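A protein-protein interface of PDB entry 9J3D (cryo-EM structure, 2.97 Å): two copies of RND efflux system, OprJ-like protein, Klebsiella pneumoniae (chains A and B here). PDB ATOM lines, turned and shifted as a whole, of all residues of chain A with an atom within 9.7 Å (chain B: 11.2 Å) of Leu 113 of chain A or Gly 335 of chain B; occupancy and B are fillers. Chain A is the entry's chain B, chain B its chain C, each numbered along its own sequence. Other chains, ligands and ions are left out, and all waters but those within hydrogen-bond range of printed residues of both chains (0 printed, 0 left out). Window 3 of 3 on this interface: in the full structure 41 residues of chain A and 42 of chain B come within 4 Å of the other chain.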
ATOM      1  N   ARG A 110     -19.853  20.957  -0.366  1.00  0.00           N
ATOM      2  CA  ARG A 110     -19.358  19.633  -0.720  1.00  0.00           C
ATOM      3  C   ARG A 110     -20.538  18.794  -1.182  1.00  0.00           C
ATOM      4  O   ARG A 110     -21.460  18.538  -0.403  1.00  0.00           O
ATOM      5  CB  ARG A 110     -18.651  18.975   0.469  1.00  0.00           C
ATOM      6  CG  ARG A 110     -17.980  17.661   0.136  1.00  0.00           C
ATOM      7  CD  ARG A 110     -16.945  17.295   1.183  1.00  0.00           C
ATOM      8  NE  ARG A 110     -16.010  16.295   0.682  1.00  0.00           N
ATOM      9  CZ  ARG A 110     -14.846  16.008   1.248  1.00  0.00           C
ATOM     10  NH1 ARG A 110     -14.441  16.620   2.348  1.00  0.00           N
ATOM     11  NH2 ARG A 110     -14.068  15.083   0.694  1.00  0.00           N
ATOM     12  N   GLN A 111     -20.508  18.370  -2.444  1.00  0.00           N
ATOM     13  CA  GLN A 111     -21.638  17.695  -3.066  1.00  0.00           C
ATOM     14  C   GLN A 111     -21.126  16.678  -4.074  1.00  0.00           C
ATOM     15  O   GLN A 111     -20.069  16.859  -4.688  1.00  0.00           O
ATOM     16  CB  GLN A 111     -22.572  18.701  -3.753  1.00  0.00           C
ATOM     17  CG  GLN A 111     -24.042  18.318  -3.758  1.00  0.00           C
ATOM     18  CD  GLN A 111     -24.378  17.256  -4.784  1.00  0.00           C
ATOM     19  OE1 GLN A 111     -24.588  16.094  -4.444  1.00  0.00           O
ATOM     20  NE2 GLN A 111     -24.432  17.653  -6.050  1.00  0.00           N
ATOM     21  N   ARG A 112     -21.893  15.596  -4.241  1.00  0.00           N
ATOM     22  CA  ARG A 112     -21.622  14.613  -5.284  1.00  0.00           C
ATOM     23  C   ARG A 112     -22.785  13.636  -5.439  1.00  0.00           C
ATOM     24  O   ARG A 112     -23.553  13.414  -4.497  1.00  0.00           O
ATOM     25  CB  ARG A 112     -20.309  13.880  -4.990  1.00  0.00           C
ATOM     26  CG  ARG A 112     -19.905  12.782  -5.971  1.00  0.00           C
ATOM     27  CD  ARG A 112     -19.895  13.182  -7.454  1.00  0.00           C
ATOM     28  NE  ARG A 112     -19.599  14.586  -7.711  1.00  0.00           N
ATOM     29  CZ  ARG A 112     -20.455  15.435  -8.264  1.00  0.00           C
ATOM     30  NH1 ARG A 112     -21.668  15.053  -8.629  1.00  0.00           N
ATOM     31  NH2 ARG A 112     -20.089  16.699  -8.451  1.00  0.00           N
ATOM     32  N   LEU A 113     -22.913  13.052  -6.630  1.00  0.00           N
ATOM     33  CA  LEU A 113     -24.107  12.285  -6.971  1.00  0.00           C
ATOM     34  C   LEU A 113     -24.168  10.895  -6.337  1.00  0.00           C
ATOM     35  O   LEU A 113     -25.274  10.480  -5.952  1.00  0.00           O
ATOM     36  CB  LEU A 113     -24.223  12.201  -8.499  1.00  0.00           C
ATOM     37  CG  LEU A 113     -25.464  11.549  -9.104  1.00  0.00           C
ATOM     38  CD1 LEU A 113     -26.446  12.620  -9.542  1.00  0.00           C
ATOM     39  CD2 LEU A 113     -25.080  10.660 -10.276  1.00  0.00           C
ATOM     40  N   PRO A 114     -23.086  10.121  -6.231  1.00  0.00           N
ATOM     41  CA  PRO A 114     -23.171   8.850  -5.498  1.00  0.00           C
ATOM     42  C   PRO A 114     -23.089   9.046  -3.991  1.00  0.00           C
ATOM     43  O   PRO A 114     -22.988  10.164  -3.480  1.00  0.00           O
ATOM     44  CB  PRO A 114     -21.972   8.048  -6.021  1.00  0.00           C
ATOM     45  CG  PRO A 114     -21.565   8.736  -7.281  1.00  0.00           C
ATOM     46  CD  PRO A 114     -21.860  10.173  -7.042  1.00  0.00           C
ATOM     47  N   ALA A 115     -23.143   7.923  -3.277  1.00  0.00           N
ATOM     48  CA  ALA A 115     -23.241   7.926  -1.824  1.00  0.00           C
ATOM     49  C   ALA A 115     -21.904   7.553  -1.183  1.00  0.00           C
ATOM     50  O   ALA A 115     -20.942   7.175  -1.859  1.00  0.00           O
ATOM     51  CB  ALA A 115     -24.346   6.977  -1.367  1.00  0.00           C
ATOM     52  N   ASP A 116     -21.863   7.642   0.153  1.00  0.00           N
ATOM     53  CA  ASP A 116     -20.655   7.525   0.969  1.00  0.00           C
ATOM     54  C   ASP A 116     -19.710   8.692   0.707  1.00  0.00           C
ATOM     55  O   ASP A 116     -20.096   9.856   0.861  1.00  0.00           O
ATOM     56  CB  ASP A 116     -19.929   6.195   0.726  1.00  0.00           C
ATOM     57  CG  ASP A 116     -20.881   5.039   0.490  1.00  0.00           C
ATOM     58  OD1 ASP A 116     -21.704   4.750   1.383  1.00  0.00           O
ATOM     59  OD2 ASP A 116     -20.802   4.418  -0.591  1.00  0.00           O
ATOM     60  N   LEU A 117     -18.474   8.376   0.324  1.00  0.00           N
ATOM     61  CA  LEU A 117     -17.448   9.347  -0.076  1.00  0.00           C
ATOM     62  C   LEU A 117     -17.345  10.531   0.892  1.00  0.00           C
ATOM     63  O   LEU A 117     -17.563  11.691   0.535  1.00  0.00           O
ATOM     64  CB  LEU A 117     -17.666   9.826  -1.517  1.00  0.00           C
ATOM     65  CG  LEU A 117     -18.777  10.769  -1.996  1.00  0.00           C
ATOM     66  CD1 LEU A 117     -18.316  11.392  -3.261  1.00  0.00           C
ATOM     67  CD2 LEU A 117     -20.073  10.071  -2.268  1.00  0.00           C
ATOM     68  N   SER A 123     -14.682   9.000  -5.401  1.00  0.00           N
ATOM     69  CA  SER A 123     -15.683   9.330  -6.409  1.00  0.00           C
ATOM     70  C   SER A 123     -15.359  10.667  -7.062  1.00  0.00           C
ATOM     71  O   SER A 123     -14.261  11.205  -6.886  1.00  0.00           O
ATOM     72  CB  SER A 123     -17.084   9.359  -5.798  1.00  0.00           C
ATOM     73  OG  SER A 123     -17.909  10.310  -6.447  1.00  0.00           O
ATOM     74  N   GLU A 124     -16.316  11.213  -7.807  1.00  0.00           N
ATOM     75  CA  GLU A 124     -16.195  12.519  -8.441  1.00  0.00           C
ATOM     76  C   GLU A 124     -16.565  13.653  -7.489  1.00  0.00           C
ATOM     77  O   GLU A 124     -17.038  14.701  -7.941  1.00  0.00           O
ATOM     78  CB  GLU A 124     -17.066  12.558  -9.709  1.00  0.00           C
ATOM     79  CG  GLU A 124     -16.808  13.714 -10.681  1.00  0.00           C
ATOM     80  CD  GLU A 124     -15.411  14.288 -10.566  1.00  0.00           C
ATOM     81  OE1 GLU A 124     -15.282  15.440 -10.100  1.00  0.00           O
ATOM     82  OE2 GLU A 124     -14.445  13.596 -10.949  1.00  0.00           O
ATOM     83  N   VAL A 125     -16.388  13.448  -6.181  1.00  0.00           N
ATOM     84  CA  VAL A 125     -16.768  14.405  -5.145  1.00  0.00           C
ATOM     85  C   VAL A 125     -16.327  15.813  -5.512  1.00  0.00           C
ATOM     86  O   VAL A 125     -15.148  16.059  -5.787  1.00  0.00           O
ATOM     87  CB  VAL A 125     -16.186  13.996  -3.778  1.00  0.00           C
ATOM     88  CG1 VAL A 125     -14.706  13.648  -3.898  1.00  0.00           C
ATOM     89  CG2 VAL A 125     -16.404  15.100  -2.752  1.00  0.00           C
ATOM     90  N   THR A 126     -17.276  16.744  -5.527  1.00  0.00           N
ATOM     91  CA  THR A 126     -16.953  18.134  -5.796  1.00  0.00           C
ATOM     92  C   THR A 126     -17.000  18.945  -4.514  1.00  0.00           C
ATOM     93  O   THR A 126     -18.010  18.968  -3.804  1.00  0.00           O
ATOM     94  CB  THR A 126     -17.911  18.727  -6.826  1.00  0.00           C
ATOM     95  OG1 THR A 126     -19.222  18.180  -6.637  1.00  0.00           O
ATOM     96  CG2 THR A 126     -17.422  18.439  -8.237  1.00  0.00           C
ATOM     97  N   SER B 127     -32.391  18.990 -18.085  1.00  0.00           N
ATOM     98  CA  SER B 127     -33.385  18.728 -17.059  1.00  0.00           C
ATOM     99  C   SER B 127     -32.716  18.016 -15.896  1.00  0.00           C
ATOM    100  O   SER B 127     -31.986  17.040 -16.088  1.00  0.00           O
ATOM    101  CB  SER B 127     -34.541  17.877 -17.602  1.00  0.00           C
ATOM    102  OG  SER B 127     -35.212  18.539 -18.659  1.00  0.00           O
ATOM    103  N   ASN B 128     -32.954  18.519 -14.690  1.00  0.00           N
ATOM    104  CA  ASN B 128     -32.495  17.867 -13.474  1.00  0.00           C
ATOM    105  C   ASN B 128     -33.670  17.719 -12.521  1.00  0.00           C
ATOM    106  O   ASN B 128     -34.557  18.577 -12.475  1.00  0.00           O
ATOM    107  CB  ASN B 128     -31.321  18.633 -12.818  1.00  0.00           C
ATOM    108  CG  ASN B 128     -31.647  20.087 -12.505  1.00  0.00           C
ATOM    109  OD1 ASN B 128     -32.715  20.409 -11.991  1.00  0.00           O
ATOM    110  ND2 ASN B 128     -30.712  20.976 -12.821  1.00  0.00           N
ATOM    111  N   TYR B 129     -33.694  16.608 -11.794  1.00  0.00           N
ATOM    112  CA  TYR B 129     -34.780  16.297 -10.877  1.00  0.00           C
ATOM    113  C   TYR B 129     -34.190  15.740  -9.593  1.00  0.00           C
ATOM    114  O   TYR B 129     -33.517  14.705  -9.611  1.00  0.00           O
ATOM    115  CB  TYR B 129     -35.762  15.304 -11.504  1.00  0.00           C
ATOM    116  CG  TYR B 129     -36.331  15.780 -12.821  1.00  0.00           C
ATOM    117  CD1 TYR B 129     -37.411  16.651 -12.857  1.00  0.00           C
ATOM    118  CD2 TYR B 129     -35.780  15.371 -14.026  1.00  0.00           C
ATOM    119  CE1 TYR B 129     -37.933  17.093 -14.058  1.00  0.00           C
ATOM    120  CE2 TYR B 129     -36.294  15.810 -15.232  1.00  0.00           C
ATOM    121  CZ  TYR B 129     -37.370  16.671 -15.242  1.00  0.00           C
ATOM    122  OH  TYR B 129     -37.887  17.110 -16.439  1.00  0.00           O
ATOM    123  N   GLN B 130     -34.440  16.432  -8.483  1.00  0.00           N
ATOM    124  CA  GLN B 130     -33.863  16.087  -7.193  1.00  0.00           C
ATOM    125  C   GLN B 130     -34.974  15.893  -6.176  1.00  0.00           C
ATOM    126  O   GLN B 130     -35.735  16.825  -5.900  1.00  0.00           O
ATOM    127  CB  GLN B 130     -32.896  17.177  -6.722  1.00  0.00           C
ATOM    128  CG  GLN B 130     -31.673  17.333  -7.606  1.00  0.00           C
ATOM    129  CD  GLN B 130     -31.053  18.711  -7.502  1.00  0.00           C
ATOM    130  OE1 GLN B 130     -31.421  19.505  -6.637  1.00  0.00           O
ATOM    131  NE2 GLN B 130     -30.108  19.003  -8.388  1.00  0.00           N
ATOM    132  N   VAL B 131     -35.063  14.689  -5.619  1.00  0.00           N
ATOM    133  CA  VAL B 131     -36.055  14.357  -4.603  1.00  0.00           C
ATOM    134  C   VAL B 131     -35.323  13.752  -3.414  1.00  0.00           C
ATOM    135  O   VAL B 131     -34.532  12.818  -3.580  1.00  0.00           O
ATOM    136  CB  VAL B 131     -37.117  13.376  -5.135  1.00  0.00           C
ATOM    137  CG1 VAL B 131     -38.025  12.909  -4.008  1.00  0.00           C
ATOM    138  CG2 VAL B 131     -37.921  14.013  -6.255  1.00  0.00           C
ATOM    139  N   SER B 320     -28.380  17.948   2.407  1.00  0.00           N
ATOM    140  CA  SER B 320     -29.364  17.211   1.628  1.00  0.00           C
ATOM    141  C   SER B 320     -28.883  15.787   1.411  1.00  0.00           C
ATOM    142  O   SER B 320     -27.684  15.522   1.326  1.00  0.00           O
ATOM    143  CB  SER B 320     -29.638  17.885   0.279  1.00  0.00           C
ATOM    144  OG  SER B 320     -28.515  17.784  -0.578  1.00  0.00           O
ATOM    145  N   VAL B 321     -29.846  14.872   1.328  1.00  0.00           N
ATOM    146  CA  VAL B 321     -29.608  13.502   0.887  1.00  0.00           C
ATOM    147  C   VAL B 321     -30.835  13.048   0.107  1.00  0.00           C
ATOM    148  O   VAL B 321     -31.971  13.275   0.535  1.00  0.00           O
ATOM    149  CB  VAL B 321     -29.301  12.550   2.063  1.00  0.00           C
ATOM    150  CG1 VAL B 321     -30.460  12.486   3.048  1.00  0.00           C
ATOM    151  CG2 VAL B 321     -28.956  11.159   1.545  1.00  0.00           C
ATOM    152  N   GLY B 322     -30.607  12.440  -1.052  1.00  0.00           N
ATOM    153  CA  GLY B 322     -31.706  12.040  -1.911  1.00  0.00           C
ATOM    154  C   GLY B 322     -31.248  11.501  -3.248  1.00  0.00           C
ATOM    155  O   GLY B 322     -30.236  10.803  -3.317  1.00  0.00           O
ATOM    156  N   SER B 323     -31.966  11.824  -4.320  1.00  0.00           N
ATOM    157  CA  SER B 323     -31.626  11.344  -5.651  1.00  0.00           C
ATOM    158  C   SER B 323     -31.534  12.513  -6.621  1.00  0.00           C
ATOM    159  O   SER B 323     -32.144  13.564  -6.413  1.00  0.00           O
ATOM    160  CB  SER B 323     -32.655  10.327  -6.162  1.00  0.00           C
ATOM    161  OG  SER B 323     -32.297   9.842  -7.445  1.00  0.00           O
ATOM    162  N   SER B 324     -30.754  12.317  -7.682  1.00  0.00           N
ATOM    163  CA  SER B 324     -30.600  13.307  -8.737  1.00  0.00           C
ATOM    164  C   SER B 324     -30.190  12.601 -10.020  1.00  0.00           C
ATOM    165  O   SER B 324     -29.432  11.628  -9.984  1.00  0.00           O
ATOM    166  CB  SER B 324     -29.559  14.371  -8.363  1.00  0.00           C
ATOM    167  OG  SER B 324     -29.547  15.426  -9.308  1.00  0.00           O
ATOM    168  N   SER B 325     -30.701  13.087 -11.149  1.00  0.00           N
ATOM    169  CA  SER B 325     -30.394  12.501 -12.445  1.00  0.00           C
ATOM    170  C   SER B 325     -30.666  13.516 -13.545  1.00  0.00           C
ATOM    171  O   SER B 325     -31.398  14.490 -13.348  1.00  0.00           O
ATOM    172  CB  SER B 325     -31.210  11.227 -12.699  1.00  0.00           C
ATOM    173  OG  SER B 325     -30.961  10.711 -13.996  1.00  0.00           O
ATOM    174  N   ALA B 326     -30.066  13.273 -14.712  1.00  0.00           N
ATOM    175  CA  ALA B 326     -30.321  14.128 -15.866  1.00  0.00           C
ATOM    176  C   ALA B 326     -31.649  13.792 -16.531  1.00  0.00           C
ATOM    177  O   ALA B 326     -32.173  14.597 -17.308  1.00  0.00           O
ATOM    178  CB  ALA B 326     -29.177  14.007 -16.873  1.00  0.00           C
ATOM    179  N   GLU B 327     -32.206  12.617 -16.244  1.00  0.00           N
ATOM    180  CA  GLU B 327     -33.485  12.202 -16.796  1.00  0.00           C
ATOM    181  C   GLU B 327     -34.346  11.610 -15.691  1.00  0.00           C
ATOM    182  O   GLU B 327     -33.837  11.086 -14.696  1.00  0.00           O
ATOM    183  CB  GLU B 327     -33.309  11.185 -17.934  1.00  0.00           C
ATOM    184  CG  GLU B 327     -32.638  11.757 -19.174  1.00  0.00           C
ATOM    185  CD  GLU B 327     -32.604  10.774 -20.327  1.00  0.00           C
ATOM    186  OE1 GLU B 327     -33.142   9.658 -20.176  1.00  0.00           O
ATOM    187  OE2 GLU B 327     -32.041  11.120 -21.388  1.00  0.00           O
ATOM    188  N   SER B 329     -36.355   8.986 -15.757  1.00  0.00           N
ATOM    189  CA  SER B 329     -36.418   7.528 -15.684  1.00  0.00           C
ATOM    190  C   SER B 329     -35.397   6.971 -14.700  1.00  0.00           C
ATOM    191  O   SER B 329     -35.645   5.949 -14.049  1.00  0.00           O
ATOM    192  CB  SER B 329     -36.201   6.926 -17.072  1.00  0.00           C
ATOM    193  OG  SER B 329     -35.134   7.569 -17.748  1.00  0.00           O
ATOM    194  N   GLY B 330     -34.248   7.628 -14.572  1.00  0.00           N
ATOM    195  CA  GLY B 330     -33.220   7.196 -13.650  1.00  0.00           C
ATOM    196  C   GLY B 330     -33.314   7.766 -12.256  1.00  0.00           C
ATOM    197  O   GLY B 330     -32.338   7.689 -11.503  1.00  0.00           O
ATOM    198  N   LEU B 331     -34.460   8.341 -11.885  1.00  0.00           N
ATOM    199  CA  LEU B 331     -34.597   8.949 -10.565  1.00  0.00           C
ATOM    200  C   LEU B 331     -34.451   7.937  -9.437  1.00  0.00           C
ATOM    201  O   LEU B 331     -33.850   8.260  -8.408  1.00  0.00           O
ATOM    202  CB  LEU B 331     -35.943   9.667 -10.452  1.00  0.00           C
ATOM    203  CG  LEU B 331     -36.169  10.471  -9.169  1.00  0.00           C
ATOM    204  CD1 LEU B 331     -35.110  11.552  -9.020  1.00  0.00           C
ATOM    205  CD2 LEU B 331     -37.562  11.077  -9.151  1.00  0.00           C
ATOM    206  N   PHE B 332     -34.986   6.724  -9.602  1.00  0.00           N
ATOM    207  CA  PHE B 332     -34.911   5.705  -8.561  1.00  0.00           C
ATOM    208  C   PHE B 332     -33.997   4.548  -8.953  1.00  0.00           C
ATOM    209  O   PHE B 332     -34.083   3.469  -8.357  1.00  0.00           O
ATOM    210  CB  PHE B 332     -36.308   5.183  -8.214  1.00  0.00           C
ATOM    211  CG  PHE B 332     -37.196   6.217  -7.584  1.00  0.00           C
ATOM    212  CD1 PHE B 332     -36.972   6.641  -6.284  1.00  0.00           C
ATOM    213  CD2 PHE B 332     -38.251   6.768  -8.290  1.00  0.00           C
ATOM    214  CE1 PHE B 332     -37.785   7.592  -5.701  1.00  0.00           C
ATOM    215  CE2 PHE B 332     -39.069   7.721  -7.712  1.00  0.00           C
ATOM    216  CZ  PHE B 332     -38.835   8.133  -6.416  1.00  0.00           C
ATOM    217  N   ASP B 333     -33.129   4.745  -9.940  1.00  0.00           N
ATOM    218  CA  ASP B 333     -32.171   3.719 -10.311  1.00  0.00           C
ATOM    219  C   ASP B 333     -30.938   3.792  -9.412  1.00  0.00           C
ATOM    220  O   ASP B 333     -30.672   4.803  -8.756  1.00  0.00           O
ATOM    221  CB  ASP B 333     -31.765   3.862 -11.777  1.00  0.00           C
ATOM    222  CG  ASP B 333     -32.876   3.465 -12.730  1.00  0.00           C
ATOM    223  OD1 ASP B 333     -33.836   2.805 -12.282  1.00  0.00           O
ATOM    224  OD2 ASP B 333     -32.787   3.812 -13.927  1.00  0.00           O
ATOM    225  N   GLY B 334     -30.187   2.695  -9.383  1.00  0.00           N
ATOM    226  CA  GLY B 334     -29.003   2.608  -8.552  1.00  0.00           C
ATOM    227  C   GLY B 334     -27.910   3.587  -8.927  1.00  0.00           C
ATOM    228  O   GLY B 334     -27.669   3.837 -10.112  1.00  0.00           O
ATOM    229  N   GLY B 335     -27.239   4.148  -7.921  1.00  0.00           N
ATOM    230  CA  GLY B 335     -26.125   5.044  -8.144  1.00  0.00           C
ATOM    231  C   GLY B 335     -26.464   6.520  -8.167  1.00  0.00           C
ATOM    232  O   GLY B 335     -25.615   7.324  -8.569  1.00  0.00           O
ATOM    233  N   SER B 336     -27.671   6.905  -7.754  1.00  0.00           N
ATOM    234  CA  SER B 336     -28.073   8.305  -7.782  1.00  0.00           C
ATOM    235  C   SER B 336     -28.186   8.930  -6.397  1.00  0.00           C
ATOM    236  O   SER B 336     -28.534  10.113  -6.300  1.00  0.00           O
ATOM    237  CB  SER B 336     -29.408   8.450  -8.519  1.00  0.00           C
ATOM    238  OG  SER B 336     -30.438   7.739  -7.855  1.00  0.00           O
ATOM    239  N   ARG B 337     -27.900   8.185  -5.332  1.00  0.00           N
ATOM    240  CA  ARG B 337     -28.063   8.712  -3.982  1.00  0.00           C
ATOM    241  C   ARG B 337     -27.013   9.777  -3.694  1.00  0.00           C
ATOM    242  O   ARG B 337     -25.857   9.461  -3.401  1.00  0.00           O
ATOM    243  CB  ARG B 337     -27.969   7.580  -2.962  1.00  0.00           C
ATOM    244  CG  ARG B 337     -28.528   7.931  -1.594  1.00  0.00           C
ATOM    245  CD  ARG B 337     -27.910   7.061  -0.516  1.00  0.00           C
ATOM    246  NE  ARG B 337     -28.142   5.643  -0.766  1.00  0.00           N
ATOM    247  CZ  ARG B 337     -27.448   4.662  -0.208  1.00  0.00           C
ATOM    248  NH1 ARG B 337     -26.461   4.907   0.639  1.00  0.00           N
ATOM    249  NH2 ARG B 337     -27.750   3.402  -0.507  1.00  0.00           N
ATOM    250  N   ALA B 338     -27.429  11.038  -3.757  1.00  0.00           N
ATOM    251  CA  ALA B 338     -26.540  12.182  -3.620  1.00  0.00           C
ATOM    252  C   ALA B 338     -26.716  12.834  -2.257  1.00  0.00           C
ATOM    253  O   ALA B 338     -27.750  12.676  -1.601  1.00  0.00           O
ATOM    254  CB  ALA B 338     -26.794  13.220  -4.721  1.00  0.00           C
ATOM    255  N   TRP B 339     -25.690  13.578  -1.845  1.00  0.00           N
ATOM    256  CA  TRP B 339     -25.716  14.300  -0.581  1.00  0.00           C
ATOM    257  C   TRP B 339     -24.970  15.617  -0.740  1.00  0.00           C
ATOM    258  O   TRP B 339     -24.170  15.798  -1.662  1.00  0.00           O
ATOM    259  CB  TRP B 339     -25.126  13.461   0.564  1.00  0.00           C
ATOM    260  CG  TRP B 339     -23.695  13.022   0.381  1.00  0.00           C
ATOM    261  CD1 TRP B 339     -23.264  11.751   0.131  1.00  0.00           C
ATOM    262  CD2 TRP B 339     -22.509  13.826   0.505  1.00  0.00           C
ATOM    263  NE1 TRP B 339     -21.893  11.720   0.052  1.00  0.00           N
ATOM    264  CE2 TRP B 339     -21.406  12.978   0.282  1.00  0.00           C
ATOM    265  CE3 TRP B 339     -22.275  15.180   0.770  1.00  0.00           C
ATOM    266  CZ2 TRP B 339     -20.093  13.440   0.310  1.00  0.00           C
ATOM    267  CZ3 TRP B 339     -20.970  15.636   0.794  1.00  0.00           C
ATOM    268  CH2 TRP B 339     -19.896  14.768   0.568  1.00  0.00           C
ATOM    269  N   SER B 340     -25.249  16.535   0.183  1.00  0.00           N
ATOM    270  CA  SER B 340     -24.665  17.867   0.178  1.00  0.00           C
ATOM    271  C   SER B 340     -24.568  18.388   1.603  1.00  0.00           C
ATOM    272  O   SER B 340     -25.475  18.181   2.413  1.00  0.00           O
ATOM    273  CB  SER B 340     -25.494  18.848  -0.660  1.00  0.00           C
ATOM    274  OG  SER B 340     -26.661  19.247   0.036  1.00  0.00           O
ATOM    275  N   PHE B 341     -23.464  19.079   1.890  1.00  0.00           N
ATOM    276  CA  PHE B 341     -23.250  19.743   3.175  1.00  0.00           C
ATOM    277  C   PHE B 341     -22.561  21.074   2.903  1.00  0.00           C
ATOM    278  O   PHE B 341     -21.556  21.117   2.188  1.00  0.00           O
ATOM    279  CB  PHE B 341     -22.415  18.878   4.119  1.00  0.00           C
ATOM    280  CG  PHE B 341     -22.100  19.542   5.430  1.00  0.00           C
ATOM    281  CD1 PHE B 341     -23.095  19.761   6.368  1.00  0.00           C
ATOM    282  CD2 PHE B 341     -20.810  19.948   5.724  1.00  0.00           C
ATOM    283  CE1 PHE B 341     -22.808  20.372   7.575  1.00  0.00           C
ATOM    284  CE2 PHE B 341     -20.516  20.559   6.930  1.00  0.00           C
ATOM    285  CZ  PHE B 341     -21.517  20.772   7.856  1.00  0.00           C
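The side-chain hydroxyl of Ser 320 of chain B lies within hydrogen-bond range of the side-chain hydroxyl of Ser 340 of chain B (2.4 Å). The backbone carbonyl oxygen (O) of Gly 322 of chain B is in hydrogen-bond range of the backbone NH (N) of Ala 338 of chain B. OG of Ser 336 of chain B is in hydrogen-bond range of O of Asp 333 of chain B (3.1 Å). OG of Ser 336 of chain B lies within hydrogen-bond range of OG of Ser 323 of chain B (2.8 Å). The backbone carbonyl oxygen (O) of Leu 331 of chain B is in hydrogen-bond range of the side-chain hydroxyl (OG) of Ser 336 of chain B. The guanidinium group of Arg 112 of chain A is in hydrogen-bond range of the backbone carbonyl oxygen of Glu 124 of chain A (2.6 Å).
Among the printed residues, merely in contact across the chains: Arg 110 of chain A with Trp 339 of chain B (3.2 Å), Arg 110 of chain A with Ser 340 of chain B (3.3 Å), Gln 111 of chain A with Ala 338 of chain B (3.6 Å), Gln 111 of chain A with Ser 340 of chain B (3.5 Å), Arg 112 of chain A with Ala 338 of chain B (3.3 Å), Leu 113 of chain A with Ser 324 of chain B (3.2 Å), Leu 113 of chain A with Gly 335 of chain B (3.8 Å), Pro 114 of chain A with Trp 339 of chain B (3.95 Å) and Leu 117 of chain A with Trp 339 of chain B (3.1 Å).
Of the 12 printed residues of chain A, 8 touch a printed residue of chain B. Hydrophobic or aromatic side chains of chain A within 4 Å of the printed part of chain B: Leu 113, Ala 115 and Leu 117. Hydrophobic or aromatic side chains of chain B within 4 Å of the printed part of chain A: Ala 338 and Trp 339. Along chain B the printed residues that touch a printed residue of chain A span positions 324 to 341. Among the printed residues, 18 pairs touch across the chains.
Leu 113 of chain A touches just these residues of chain B: Ser 324 (3.2 Å), Gly 335 (3.8 Å), Ser 336 (3.3 Å), Arg 337 (2.8 Å) and Ala 338 (3.1 Å). Gly 335 of chain B touches just one residue of chain A: Leu 113. Ala 115 of chain A touches just one residue of chain B: Arg 337 (3.1 Å). Ser 324 of chain B touches just one residue of chain A: Leu 113. No residue of chain A comes within 4 Å of Gly 334 of chain B. Of chain A, only Gln 111, Arg 112 and Leu 113 come within 4 Å of Ala 338 of chain B. Of the printed residues of chain A, Trp 339 of chain B touches Arg 110 (3.2 Å), Gln 111 (2.8 Å), Arg 112 (3.4 Å), Pro 114 (3.95 Å), Asp 116 (2.7 Å) and Leu 117 (3.1 Å). Of the printed residues of chain B, Leu 117 of chain A touches Trp 339. Printed residues of chain B within 4 Å of Asp 116 of chain A: Trp 339. The nearest residue of chain B that does not touch Leu 113 of chain A is Ser 325 of chain B (4.6 Å).
O of Arg 337 of chain B lies close to O of Leu 113 of chain A. The backbone carbonyl oxygen (O) of Leu 113 of chain A lies close to the backbone carbonyl oxygen (O) of Ser 336 of chain B (3.3 Å). The backbone NH of Arg 110 of chain A is in hydrogen-bond range of the backbone carbonyl oxygen of Phe 341 of chain B. The backbone carbonyl oxygen (O) of Pro 114 of chain A lies close to the backbone carbonyl oxygen (O) of Arg 337 of chain B, at 3.0 Å. O of Leu 113 of chain A is in hydrogen-bond range of N of Ala 338 of chain B, at 3.1 Å. The backbone NH (N) of Ala 115 of chain A is in hydrogen-bond range of the backbone carbonyl oxygen (O) of Arg 337 of chain B (3.1 Å). O of Arg 112 of chain A is in hydrogen-bond range of N of Trp 339 of chain B (3.4 Å). O of Asp 116 of chain A is in hydrogen-bond range of NE1 of Trp 339 of chain B. The side-chain amide oxygen of Gln 111 of chain A lies close to the backbone carbonyl oxygen of Trp 339 of chain B (2.8 Å).
No position is printed for both chains. Of the 18 pairs that touch across the chains among the printed residues, none has its exchanged pair printed and touching as well.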
